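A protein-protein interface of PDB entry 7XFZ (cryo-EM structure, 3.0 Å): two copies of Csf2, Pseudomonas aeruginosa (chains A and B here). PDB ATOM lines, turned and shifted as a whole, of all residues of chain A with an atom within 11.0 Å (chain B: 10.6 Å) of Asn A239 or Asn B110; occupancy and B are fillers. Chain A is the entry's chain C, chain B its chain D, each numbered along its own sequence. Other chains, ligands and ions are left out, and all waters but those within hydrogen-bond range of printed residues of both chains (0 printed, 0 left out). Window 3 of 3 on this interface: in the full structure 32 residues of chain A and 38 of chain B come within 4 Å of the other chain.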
ATOM      1  N   ARG A 181      17.808  20.500   1.012  1.00  0.00           N
ATOM      2  CA  ARG A 181      18.594  19.312   0.704  1.00  0.00           C
ATOM      3  C   ARG A 181      17.845  18.093   1.219  1.00  0.00           C
ATOM      4  O   ARG A 181      17.281  18.130   2.314  1.00  0.00           O
ATOM      5  CB  ARG A 181      19.999  19.371   1.315  1.00  0.00           C
ATOM      6  CG  ARG A 181      20.874  18.194   0.905  1.00  0.00           C
ATOM      7  CD  ARG A 181      22.328  18.369   1.303  1.00  0.00           C
ATOM      8  NE  ARG A 181      22.520  18.385   2.745  1.00  0.00           N
ATOM      9  CZ  ARG A 181      23.655  18.719   3.343  1.00  0.00           C
ATOM     10  NH1 ARG A 181      24.723  19.070   2.647  1.00  0.00           N
ATOM     11  NH2 ARG A 181      23.720  18.697   4.669  1.00  0.00           N
ATOM     12  N   TRP A 207      21.245   1.937   6.949  1.00  0.00           N
ATOM     13  CA  TRP A 207      21.293   3.396   6.996  1.00  0.00           C
ATOM     14  C   TRP A 207      20.083   3.960   7.735  1.00  0.00           C
ATOM     15  O   TRP A 207      20.217   4.840   8.601  1.00  0.00           O
ATOM     16  CB  TRP A 207      21.370   3.933   5.565  1.00  0.00           C
ATOM     17  CG  TRP A 207      21.447   5.422   5.406  1.00  0.00           C
ATOM     18  CD1 TRP A 207      20.438   6.322   5.578  1.00  0.00           C
ATOM     19  CD2 TRP A 207      22.591   6.178   4.988  1.00  0.00           C
ATOM     20  NE1 TRP A 207      20.887   7.592   5.317  1.00  0.00           N
ATOM     21  CE2 TRP A 207      22.205   7.531   4.952  1.00  0.00           C
ATOM     22  CE3 TRP A 207      23.906   5.842   4.654  1.00  0.00           C
ATOM     23  CZ2 TRP A 207      23.088   8.546   4.595  1.00  0.00           C
ATOM     24  CZ3 TRP A 207      24.778   6.851   4.299  1.00  0.00           C
ATOM     25  CH2 TRP A 207      24.367   8.187   4.273  1.00  0.00           C
ATOM     26  N   LEU A 211      19.916   6.064  11.344  1.00  0.00           N
ATOM     27  CA  LEU A 211      19.170   7.307  11.529  1.00  0.00           C
ATOM     28  C   LEU A 211      18.204   7.201  12.705  1.00  0.00           C
ATOM     29  O   LEU A 211      18.149   8.095  13.561  1.00  0.00           O
ATOM     30  CB  LEU A 211      18.410   7.668  10.254  1.00  0.00           C
ATOM     31  CG  LEU A 211      19.219   8.220   9.082  1.00  0.00           C
ATOM     32  CD1 LEU A 211      18.290   8.598   7.943  1.00  0.00           C
ATOM     33  CD2 LEU A 211      20.040   9.418   9.520  1.00  0.00           C
ATOM     34  N   ASN A 214      20.117   7.095  16.114  1.00  0.00           N
ATOM     35  CA  ASN A 214      20.617   8.414  16.489  1.00  0.00           C
ATOM     36  C   ASN A 214      19.485   9.315  16.962  1.00  0.00           C
ATOM     37  O   ASN A 214      19.632  10.039  17.955  1.00  0.00           O
ATOM     38  CB  ASN A 214      21.357   9.048  15.313  1.00  0.00           C
ATOM     39  CG  ASN A 214      22.737   8.457  15.106  1.00  0.00           C
ATOM     40  OD1 ASN A 214      23.042   7.374  15.605  1.00  0.00           O
ATOM     41  ND2 ASN A 214      23.582   9.168  14.369  1.00  0.00           N
ATOM     42  N   SER A 215      18.344   9.283  16.267  1.00  0.00           N
ATOM     43  CA  SER A 215      17.205  10.096  16.681  1.00  0.00           C
ATOM     44  C   SER A 215      16.710   9.684  18.063  1.00  0.00           C
ATOM     45  O   SER A 215      16.397  10.536  18.902  1.00  0.00           O
ATOM     46  CB  SER A 215      16.082   9.989  15.652  1.00  0.00           C
ATOM     47  OG  SER A 215      14.824  10.256  16.247  1.00  0.00           O
ATOM     48  N   ALA A 217      18.451   8.182  20.484  1.00  0.00           N
ATOM     49  CA  ALA A 217      19.430   8.578  21.489  1.00  0.00           C
ATOM     50  C   ALA A 217      19.345  10.070  21.782  1.00  0.00           C
ATOM     51  O   ALA A 217      19.372  10.484  22.947  1.00  0.00           O
ATOM     52  CB  ALA A 217      20.837   8.198  21.031  1.00  0.00           C
ATOM     53  N   ALA A 218      19.231  10.892  20.735  1.00  0.00           N
ATOM     54  CA  ALA A 218      19.120  12.332  20.943  1.00  0.00           C
ATOM     55  C   ALA A 218      17.848  12.685  21.704  1.00  0.00           C
ATOM     56  O   ALA A 218      17.875  13.523  22.614  1.00  0.00           O
ATOM     57  CB  ALA A 218      19.166  13.063  19.602  1.00  0.00           C
ATOM     58  N   ALA A 219      16.726  12.053  21.353  1.00  0.00           N
ATOM     59  CA  ALA A 219      15.469  12.342  22.034  1.00  0.00           C
ATOM     60  C   ALA A 219      15.528  11.936  23.501  1.00  0.00           C
ATOM     61  O   ALA A 219      14.993  12.637  24.368  1.00  0.00           O
ATOM     62  CB  ALA A 219      14.314  11.633  21.326  1.00  0.00           C
ATOM     63  N   LYS A 221      18.293  11.815  25.316  1.00  0.00           N
ATOM     64  CA  LYS A 221      19.213  12.729  25.988  1.00  0.00           C
ATOM     65  C   LYS A 221      18.558  14.080  26.255  1.00  0.00           C
ATOM     66  O   LYS A 221      18.821  14.710  27.286  1.00  0.00           O
ATOM     67  CB  LYS A 221      20.483  12.892  25.150  1.00  0.00           C
ATOM     68  CG  LYS A 221      21.654  13.560  25.869  1.00  0.00           C
ATOM     69  CD  LYS A 221      21.655  15.072  25.694  1.00  0.00           C
ATOM     70  CE  LYS A 221      22.988  15.673  26.101  1.00  0.00           C
ATOM     71  NZ  LYS A 221      23.027  17.143  25.875  1.00  0.00           N
ATOM     72  N   LYS A 222      17.710  14.546  25.333  1.00  0.00           N
ATOM     73  CA  LYS A 222      17.104  15.868  25.483  1.00  0.00           C
ATOM     74  C   LYS A 222      16.245  15.954  26.739  1.00  0.00           C
ATOM     75  O   LYS A 222      16.300  16.950  27.468  1.00  0.00           O
ATOM     76  CB  LYS A 222      16.274  16.213  24.246  1.00  0.00           C
ATOM     77  CG  LYS A 222      17.096  16.538  23.010  1.00  0.00           C
ATOM     78  CD  LYS A 222      17.894  17.817  23.195  1.00  0.00           C
ATOM     79  CE  LYS A 222      16.978  19.016  23.384  1.00  0.00           C
ATOM     80  NZ  LYS A 222      17.744  20.280  23.559  1.00  0.00           N
ATOM     81  N   ASN A 239      28.110  17.929  16.817  1.00  0.00           N
ATOM     82  CA  ASN A 239      27.600  16.564  16.877  1.00  0.00           C
ATOM     83  C   ASN A 239      27.260  16.050  15.483  1.00  0.00           C
ATOM     84  O   ASN A 239      27.355  16.788  14.503  1.00  0.00           O
ATOM     85  CB  ASN A 239      26.371  16.491  17.783  1.00  0.00           C
ATOM     86  CG  ASN A 239      26.685  15.898  19.142  1.00  0.00           C
ATOM     87  OD1 ASN A 239      27.848  15.696  19.489  1.00  0.00           O
ATOM     88  ND2 ASN A 239      25.646  15.620  19.920  1.00  0.00           N
ATOM     89  N   GLY A 240      26.870  14.780  15.403  1.00  0.00           N
ATOM     90  CA  GLY A 240      26.531  14.204  14.113  1.00  0.00           C
ATOM     91  C   GLY A 240      25.353  14.924  13.481  1.00  0.00           C
ATOM     92  O   GLY A 240      24.415  15.342  14.162  1.00  0.00           O
ATOM     93  N   ARG A 241      25.408  15.069  12.161  1.00  0.00           N
ATOM     94  CA  ARG A 241      24.398  15.799  11.414  1.00  0.00           C
ATOM     95  C   ARG A 241      23.994  14.999  10.187  1.00  0.00           C
ATOM     96  O   ARG A 241      24.848  14.451   9.483  1.00  0.00           O
ATOM     97  CB  ARG A 241      24.916  17.181  11.003  1.00  0.00           C
ATOM     98  CG  ARG A 241      23.997  17.941  10.078  1.00  0.00           C
ATOM     99  CD  ARG A 241      23.753  19.355  10.566  1.00  0.00           C
ATOM    100  NE  ARG A 241      23.161  20.175   9.516  1.00  0.00           N
ATOM    101  CZ  ARG A 241      21.885  20.533   9.473  1.00  0.00           C
ATOM    102  NH1 ARG A 241      21.037  20.184  10.425  1.00  0.00           N
ATOM    103  NH2 ARG A 241      21.450  21.260   8.450  1.00  0.00           N
ATOM    104  N   GLY A 242      22.692  14.931   9.934  1.00  0.00           N
ATOM    105  CA  GLY A 242      22.163  14.225   8.784  1.00  0.00           C
ATOM    106  C   GLY A 242      22.250  15.047   7.518  1.00  0.00           C
ATOM    107  O   GLY A 242      22.954  16.060   7.451  1.00  0.00           O
ATOM    108  N   LEU A 243      21.514  14.613   6.496  1.00  0.00           N
ATOM    109  CA  LEU A 243      21.576  15.236   5.185  1.00  0.00           C
ATOM    110  C   LEU A 243      20.416  16.175   4.886  1.00  0.00           C
ATOM    111  O   LEU A 243      20.517  16.962   3.941  1.00  0.00           O
ATOM    112  CB  LEU A 243      21.644  14.162   4.090  1.00  0.00           C
ATOM    113  CG  LEU A 243      23.045  13.742   3.643  1.00  0.00           C
ATOM    114  CD1 LEU A 243      22.967  12.696   2.548  1.00  0.00           C
ATOM    115  CD2 LEU A 243      23.840  14.944   3.175  1.00  0.00           C
ATOM    116  N   LYS A 244      19.328  16.119   5.648  1.00  0.00           N
ATOM    117  CA  LYS A 244      18.227  17.051   5.452  1.00  0.00           C
ATOM    118  C   LYS A 244      18.637  18.457   5.873  1.00  0.00           C
ATOM    119  O   LYS A 244      19.403  18.636   6.823  1.00  0.00           O
ATOM    120  CB  LYS A 244      17.005  16.600   6.249  1.00  0.00           C
ATOM    121  CG  LYS A 244      15.885  16.021   5.408  1.00  0.00           C
ATOM    122  CD  LYS A 244      14.622  15.838   6.231  1.00  0.00           C
ATOM    123  CE  LYS A 244      13.553  16.844   5.829  1.00  0.00           C
ATOM    124  NZ  LYS A 244      12.195  16.457   6.304  1.00  0.00           N
ATOM    125  N   ALA A 245      18.125  19.459   5.160  1.00  0.00           N
ATOM    126  CA  ALA A 245      18.479  20.842   5.445  1.00  0.00           C
ATOM    127  C   ALA A 245      17.412  21.770   4.887  1.00  0.00           C
ATOM    128  O   ALA A 245      16.662  21.401   3.982  1.00  0.00           O
ATOM    129  CB  ALA A 245      19.848  21.201   4.860  1.00  0.00           C
ATOM    130  N   GLY B 105      25.631  15.162  -3.243  1.00  0.00           N
ATOM    131  CA  GLY B 105      26.830  15.905  -2.916  1.00  0.00           C
ATOM    132  C   GLY B 105      27.615  15.291  -1.777  1.00  0.00           C
ATOM    133  O   GLY B 105      28.439  14.406  -1.997  1.00  0.00           O
ATOM    134  N   ASN B 106      27.399  15.778  -0.558  1.00  0.00           N
ATOM    135  CA  ASN B 106      28.054  15.203   0.608  1.00  0.00           C
ATOM    136  C   ASN B 106      27.336  13.935   1.059  1.00  0.00           C
ATOM    137  O   ASN B 106      26.179  13.703   0.704  1.00  0.00           O
ATOM    138  CB  ASN B 106      28.094  16.229   1.739  1.00  0.00           C
ATOM    139  CG  ASN B 106      29.279  16.035   2.662  1.00  0.00           C
ATOM    140  OD1 ASN B 106      30.027  15.065   2.537  1.00  0.00           O
ATOM    141  ND2 ASN B 106      29.457  16.962   3.598  1.00  0.00           N
ATOM    142  N   ALA B 107      28.036  13.104   1.835  1.00  0.00           N
ATOM    143  CA  ALA B 107      27.419  11.894   2.375  1.00  0.00           C
ATOM    144  C   ALA B 107      26.978  12.092   3.819  1.00  0.00           C
ATOM    145  O   ALA B 107      26.179  11.308   4.341  1.00  0.00           O
ATOM    146  CB  ALA B 107      28.383  10.716   2.273  1.00  0.00           C
ATOM    147  N   THR B 108      27.501  13.117   4.485  1.00  0.00           N
ATOM    148  CA  THR B 108      27.146  13.429   5.859  1.00  0.00           C
ATOM    149  C   THR B 108      26.913  14.928   6.006  1.00  0.00           C
ATOM    150  O   THR B 108      27.068  15.699   5.057  1.00  0.00           O
ATOM    151  CB  THR B 108      28.233  12.967   6.838  1.00  0.00           C
ATOM    152  OG1 THR B 108      27.911  13.417   8.159  1.00  0.00           O
ATOM    153  CG2 THR B 108      29.584  13.524   6.434  1.00  0.00           C
ATOM    154  N   GLY B 109      26.524  15.331   7.214  1.00  0.00           N
ATOM    155  CA  GLY B 109      26.218  16.732   7.450  1.00  0.00           C
ATOM    156  C   GLY B 109      27.429  17.556   7.843  1.00  0.00           C
ATOM    157  O   GLY B 109      27.424  18.781   7.713  1.00  0.00           O
ATOM    158  N   ASN B 110      28.477  16.901   8.344  1.00  0.00           N
ATOM    159  CA  ASN B 110      29.639  17.644   8.824  1.00  0.00           C
ATOM    160  C   ASN B 110      30.818  17.461   7.877  1.00  0.00           C
ATOM    161  O   ASN B 110      31.282  16.332   7.689  1.00  0.00           O
ATOM    162  CB  ASN B 110      30.036  17.190  10.220  1.00  0.00           C
ATOM    163  CG  ASN B 110      28.845  16.932  11.108  1.00  0.00           C
ATOM    164  OD1 ASN B 110      28.233  15.870  11.048  1.00  0.00           O
ATOM    165  ND2 ASN B 110      28.506  17.906  11.941  1.00  0.00           N
ATOM    166  N   PRO B 111      31.332  18.531   7.274  1.00  0.00           N
ATOM    167  CA  PRO B 111      32.533  18.402   6.444  1.00  0.00           C
ATOM    168  C   PRO B 111      33.813  18.511   7.256  1.00  0.00           C
ATOM    169  O   PRO B 111      33.904  19.335   8.170  1.00  0.00           O
ATOM    170  CB  PRO B 111      32.394  19.568   5.462  1.00  0.00           C
ATOM    171  CG  PRO B 111      31.678  20.615   6.247  1.00  0.00           C
ATOM    172  CD  PRO B 111      30.802  19.906   7.260  1.00  0.00           C
ATOM    173  N   ASP B 112      34.806  17.683   6.942  1.00  0.00           N
ATOM    174  CA  ASP B 112      36.102  17.820   7.590  1.00  0.00           C
ATOM    175  C   ASP B 112      36.811  19.067   7.079  1.00  0.00           C
ATOM    176  O   ASP B 112      36.768  19.382   5.886  1.00  0.00           O
ATOM    177  CB  ASP B 112      36.959  16.579   7.347  1.00  0.00           C
ATOM    178  CG  ASP B 112      36.778  16.012   5.960  1.00  0.00           C
ATOM    179  OD1 ASP B 112      36.049  16.631   5.162  1.00  0.00           O
ATOM    180  OD2 ASP B 112      37.362  14.948   5.668  1.00  0.00           O
ATOM    181  N   GLY B 113      37.466  19.779   7.989  1.00  0.00           N
ATOM    182  CA  GLY B 113      38.123  21.019   7.642  1.00  0.00           C
ATOM    183  C   GLY B 113      39.476  20.876   6.994  1.00  0.00           C
ATOM    184  O   GLY B 113      40.112  21.885   6.678  1.00  0.00           O
ATOM    185  N   VAL B 114      39.939  19.649   6.787  1.00  0.00           N
ATOM    186  CA  VAL B 114      41.243  19.395   6.182  1.00  0.00           C
ATOM    187  C   VAL B 114      41.181  19.719   4.694  1.00  0.00           C
ATOM    188  O   VAL B 114      40.094  19.688   4.096  1.00  0.00           O
ATOM    189  CB  VAL B 114      41.689  17.944   6.423  1.00  0.00           C
ATOM    190  CG1 VAL B 114      41.400  17.534   7.857  1.00  0.00           C
ATOM    191  CG2 VAL B 114      40.999  17.001   5.451  1.00  0.00           C
ATOM    192  N   GLY B 135      31.547  18.894  -4.786  1.00  0.00           N
ATOM    193  CA  GLY B 135      31.070  18.459  -3.490  1.00  0.00           C
ATOM    194  C   GLY B 135      32.044  17.562  -2.760  1.00  0.00           C
ATOM    195  O   GLY B 135      33.257  17.779  -2.814  1.00  0.00           O
ATOM    196  N   GLY B 136      31.525  16.549  -2.075  1.00  0.00           N
ATOM    197  CA  GLY B 136      32.351  15.627  -1.337  1.00  0.00           C
ATOM    198  C   GLY B 136      32.686  16.139   0.046  1.00  0.00           C
ATOM    199  O   GLY B 136      32.279  17.233   0.444  1.00  0.00           O
ATOM    200  N   PRO B 137      33.433  15.344   0.814  1.00  0.00           N
ATOM    201  CA  PRO B 137      33.807  15.776   2.169  1.00  0.00           C
ATOM    202  C   PRO B 137      34.623  17.053   2.194  1.00  0.00           C
ATOM    203  O   PRO B 137      34.487  17.845   3.134  1.00  0.00           O
ATOM    204  CB  PRO B 137      34.613  14.585   2.706  1.00  0.00           C
ATOM    205  CG  PRO B 137      34.231  13.435   1.845  1.00  0.00           C
ATOM    206  CD  PRO B 137      33.954  14.006   0.496  1.00  0.00           C
ATOM    207  N   ARG B 138      35.465  17.279   1.190  1.00  0.00           N
ATOM    208  CA  ARG B 138      36.360  18.426   1.149  1.00  0.00           C
ATOM    209  C   ARG B 138      35.840  19.551   0.262  1.00  0.00           C
ATOM    210  O   ARG B 138      36.569  20.515   0.013  1.00  0.00           O
ATOM    211  CB  ARG B 138      37.745  17.984   0.680  1.00  0.00           C
ATOM    212  CG  ARG B 138      38.643  17.487   1.796  1.00  0.00           C
ATOM    213  CD  ARG B 138      39.377  16.231   1.378  1.00  0.00           C
ATOM    214  NE  ARG B 138      38.778  15.032   1.949  1.00  0.00           N
ATOM    215  CZ  ARG B 138      38.778  13.844   1.363  1.00  0.00           C
ATOM    216  NH1 ARG B 138      39.318  13.663   0.170  1.00  0.00           N
ATOM    217  NH2 ARG B 138      38.217  12.813   1.986  1.00  0.00           N
ATOM    218  N   MET B 139      34.604  19.443  -0.222  1.00  0.00           N
ATOM    219  CA  MET B 139      33.924  20.513  -0.953  1.00  0.00           C
ATOM    220  C   MET B 139      34.692  20.915  -2.212  1.00  0.00           C
ATOM    221  O   MET B 139      35.170  22.041  -2.349  1.00  0.00           O
ATOM    222  CB  MET B 139      33.686  21.721  -0.046  1.00  0.00           C
ATOM    223  CG  MET B 139      32.399  21.631   0.749  1.00  0.00           C
ATOM    224  SD  MET B 139      31.758  23.231   1.248  1.00  0.00           S
ATOM    225  CE  MET B 139      31.499  22.960   2.999  1.00  0.00           C
ATOM    226  N   ALA B 342      34.213   9.748  -2.360  1.00  0.00           N
ATOM    227  CA  ALA B 342      33.275   9.762  -1.244  1.00  0.00           C
ATOM    228  C   ALA B 342      33.955   9.540   0.098  1.00  0.00           C
ATOM    229  O   ALA B 342      33.408   9.953   1.124  1.00  0.00           O
ATOM    230  CB  ALA B 342      32.195   8.703  -1.453  1.00  0.00           C
ATOM    231  N   GLN B 343      35.118   8.895   0.114  1.00  0.00           N
ATOM    232  CA  GLN B 343      35.788   8.575   1.368  1.00  0.00           C
ATOM    233  C   GLN B 343      36.189   9.849   2.099  1.00  0.00           C
ATOM    234  O   GLN B 343      36.742  10.774   1.500  1.00  0.00           O
ATOM    235  CB  GLN B 343      37.016   7.708   1.105  1.00  0.00           C
ATOM    236  CG  GLN B 343      37.313   6.708   2.206  1.00  0.00           C
ATOM    237  CD  GLN B 343      38.448   7.151   3.104  1.00  0.00           C
ATOM    238  OE1 GLN B 343      39.360   7.853   2.670  1.00  0.00           O
ATOM    239  NE2 GLN B 343      38.401   6.738   4.365  1.00  0.00           N
ATOM    240  N   SER B 344      35.913   9.891   3.397  1.00  0.00           N
ATOM    241  CA  SER B 344      36.239  11.035   4.235  1.00  0.00           C
ATOM    242  C   SER B 344      37.455  10.709   5.091  1.00  0.00           C
ATOM    243  O   SER B 344      37.443   9.736   5.852  1.00  0.00           O
ATOM    244  CB  SER B 344      35.056  11.413   5.124  1.00  0.00           C
ATOM    245  OG  SER B 344      34.995  10.585   6.270  1.00  0.00           O
ATOM    246  N   ALA B 345      38.497  11.526   4.968  1.00  0.00           N
ATOM    247  CA  ALA B 345      39.731  11.327   5.724  1.00  0.00           C
ATOM    248  C   ALA B 345      39.711  12.199   6.977  1.00  0.00           C
ATOM    249  O   ALA B 345      40.525  13.104   7.166  1.00  0.00           O
ATOM    250  CB  ALA B 345      40.943  11.628   4.848  1.00  0.00           C
ATOM    251  N   LYS B 346      38.752  11.900   7.846  1.00  0.00           N
ATOM    252  CA  LYS B 346      38.601  12.636   9.096  1.00  0.00           C
ATOM    253  C   LYS B 346      39.509  12.062  10.179  1.00  0.00           C
ATOM    254  O   LYS B 346      40.731  12.191  10.109  1.00  0.00           O
ATOM    255  CB  LYS B 346      37.145  12.613   9.565  1.00  0.00           C
ATOM    256  CG  LYS B 346      36.772  13.773  10.472  1.00  0.00           C
ATOM    257  CD  LYS B 346      35.267  13.876  10.648  1.00  0.00           C
ATOM    258  CE  LYS B 346      34.583  14.339   9.374  1.00  0.00           C
ATOM    259  NZ  LYS B 346      33.240  14.912   9.652  1.00  0.00           N
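The side-chain amide nitrogen (ND2) of Asn B110 is in hydrogen-bond range of the backbone carbonyl oxygen (O) of Asn A239.
The side-chain hydroxyl (OG1) of Thr B108 lies within hydrogen-bond range of the backbone carbonyl oxygen (O) of Arg A241 (3.5 Å).
The backbone carbonyl oxygen (O) of Arg A241 lies within hydrogen-bond range of the backbone NH (N) of Gly B109 (3.0 Å).
The backbone NH of Arg A241 is in hydrogen-bond range of the side-chain amide oxygen of Asn B110.
The guanidinium group (NE) of Arg A181 sits at hydrogen-bond distance from the backbone carbonyl oxygen (O) of Leu A243 (2.7 Å).
The side-chain amide nitrogen of Asn B106 lies within hydrogen-bond range of the backbone carbonyl oxygen of Thr B108 (3.1 Å).
O of Asn B110 sits at hydrogen-bond distance from NZ of Lys B346 (3.1 Å).
Trp A207 touches Ala B107.
Asn B110 touches Gly A240.
Gly A242 touches Gly B109.
Leu A243 touches Asn B106 (CD2 to O, 3.6 Å).
Leu A243 touches Ala B107.
Leu A243 touches Thr B108.
Of chain A, only Asn A239 (3.0 Å), Gly A240 (3.9 Å) and Arg A241 (3.1 Å) come within 4 Å of Asn B110.
Gly A240 touches just one residue of chain B: Asn B110.
Thr B108 touches two residues of chain A.
Of chain A, only Arg A241 and Gly A242 come within 4 Å of Gly B109.
No residue of chain A comes within 4 Å of Asp B112.
Printed residues of chain B within 4 Å of Arg A241: Thr B108, Gly B109 and Asn B110.
Printed residues of chain A within 4 Å of Ala B107: Trp A207 (3.6 Å) and Leu A243 (3.9 Å).
Of the printed residues of chain A, Asn B106 touches Leu A243.
Gly B136 touches none of the printed residues of chain A.
The nearest residue of chain B that does not touch Asn A239 is Gly B109 (6.7 Å).
The nearest printed residue of chain A that does not touch Ala B107 is Arg A241 (6.2 Å).
Hydrophobic or aromatic side chains of chain A within 4 Å of the printed part of chain B: Trp A207 and Leu A243.
Of the 20 printed residues of chain B, 5 touch a printed residue of chain A.
Printed residues of chain B that touch a printed residue of chain A: Asn B106, Ala B107, Thr B108, Gly B109 and Asn B110.
Among the printed residues, no Asp or Glu carboxylate lies within 4 Å of a Lys or Arg side-chain nitrogen of the other chain.
No position is printed for both chains.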
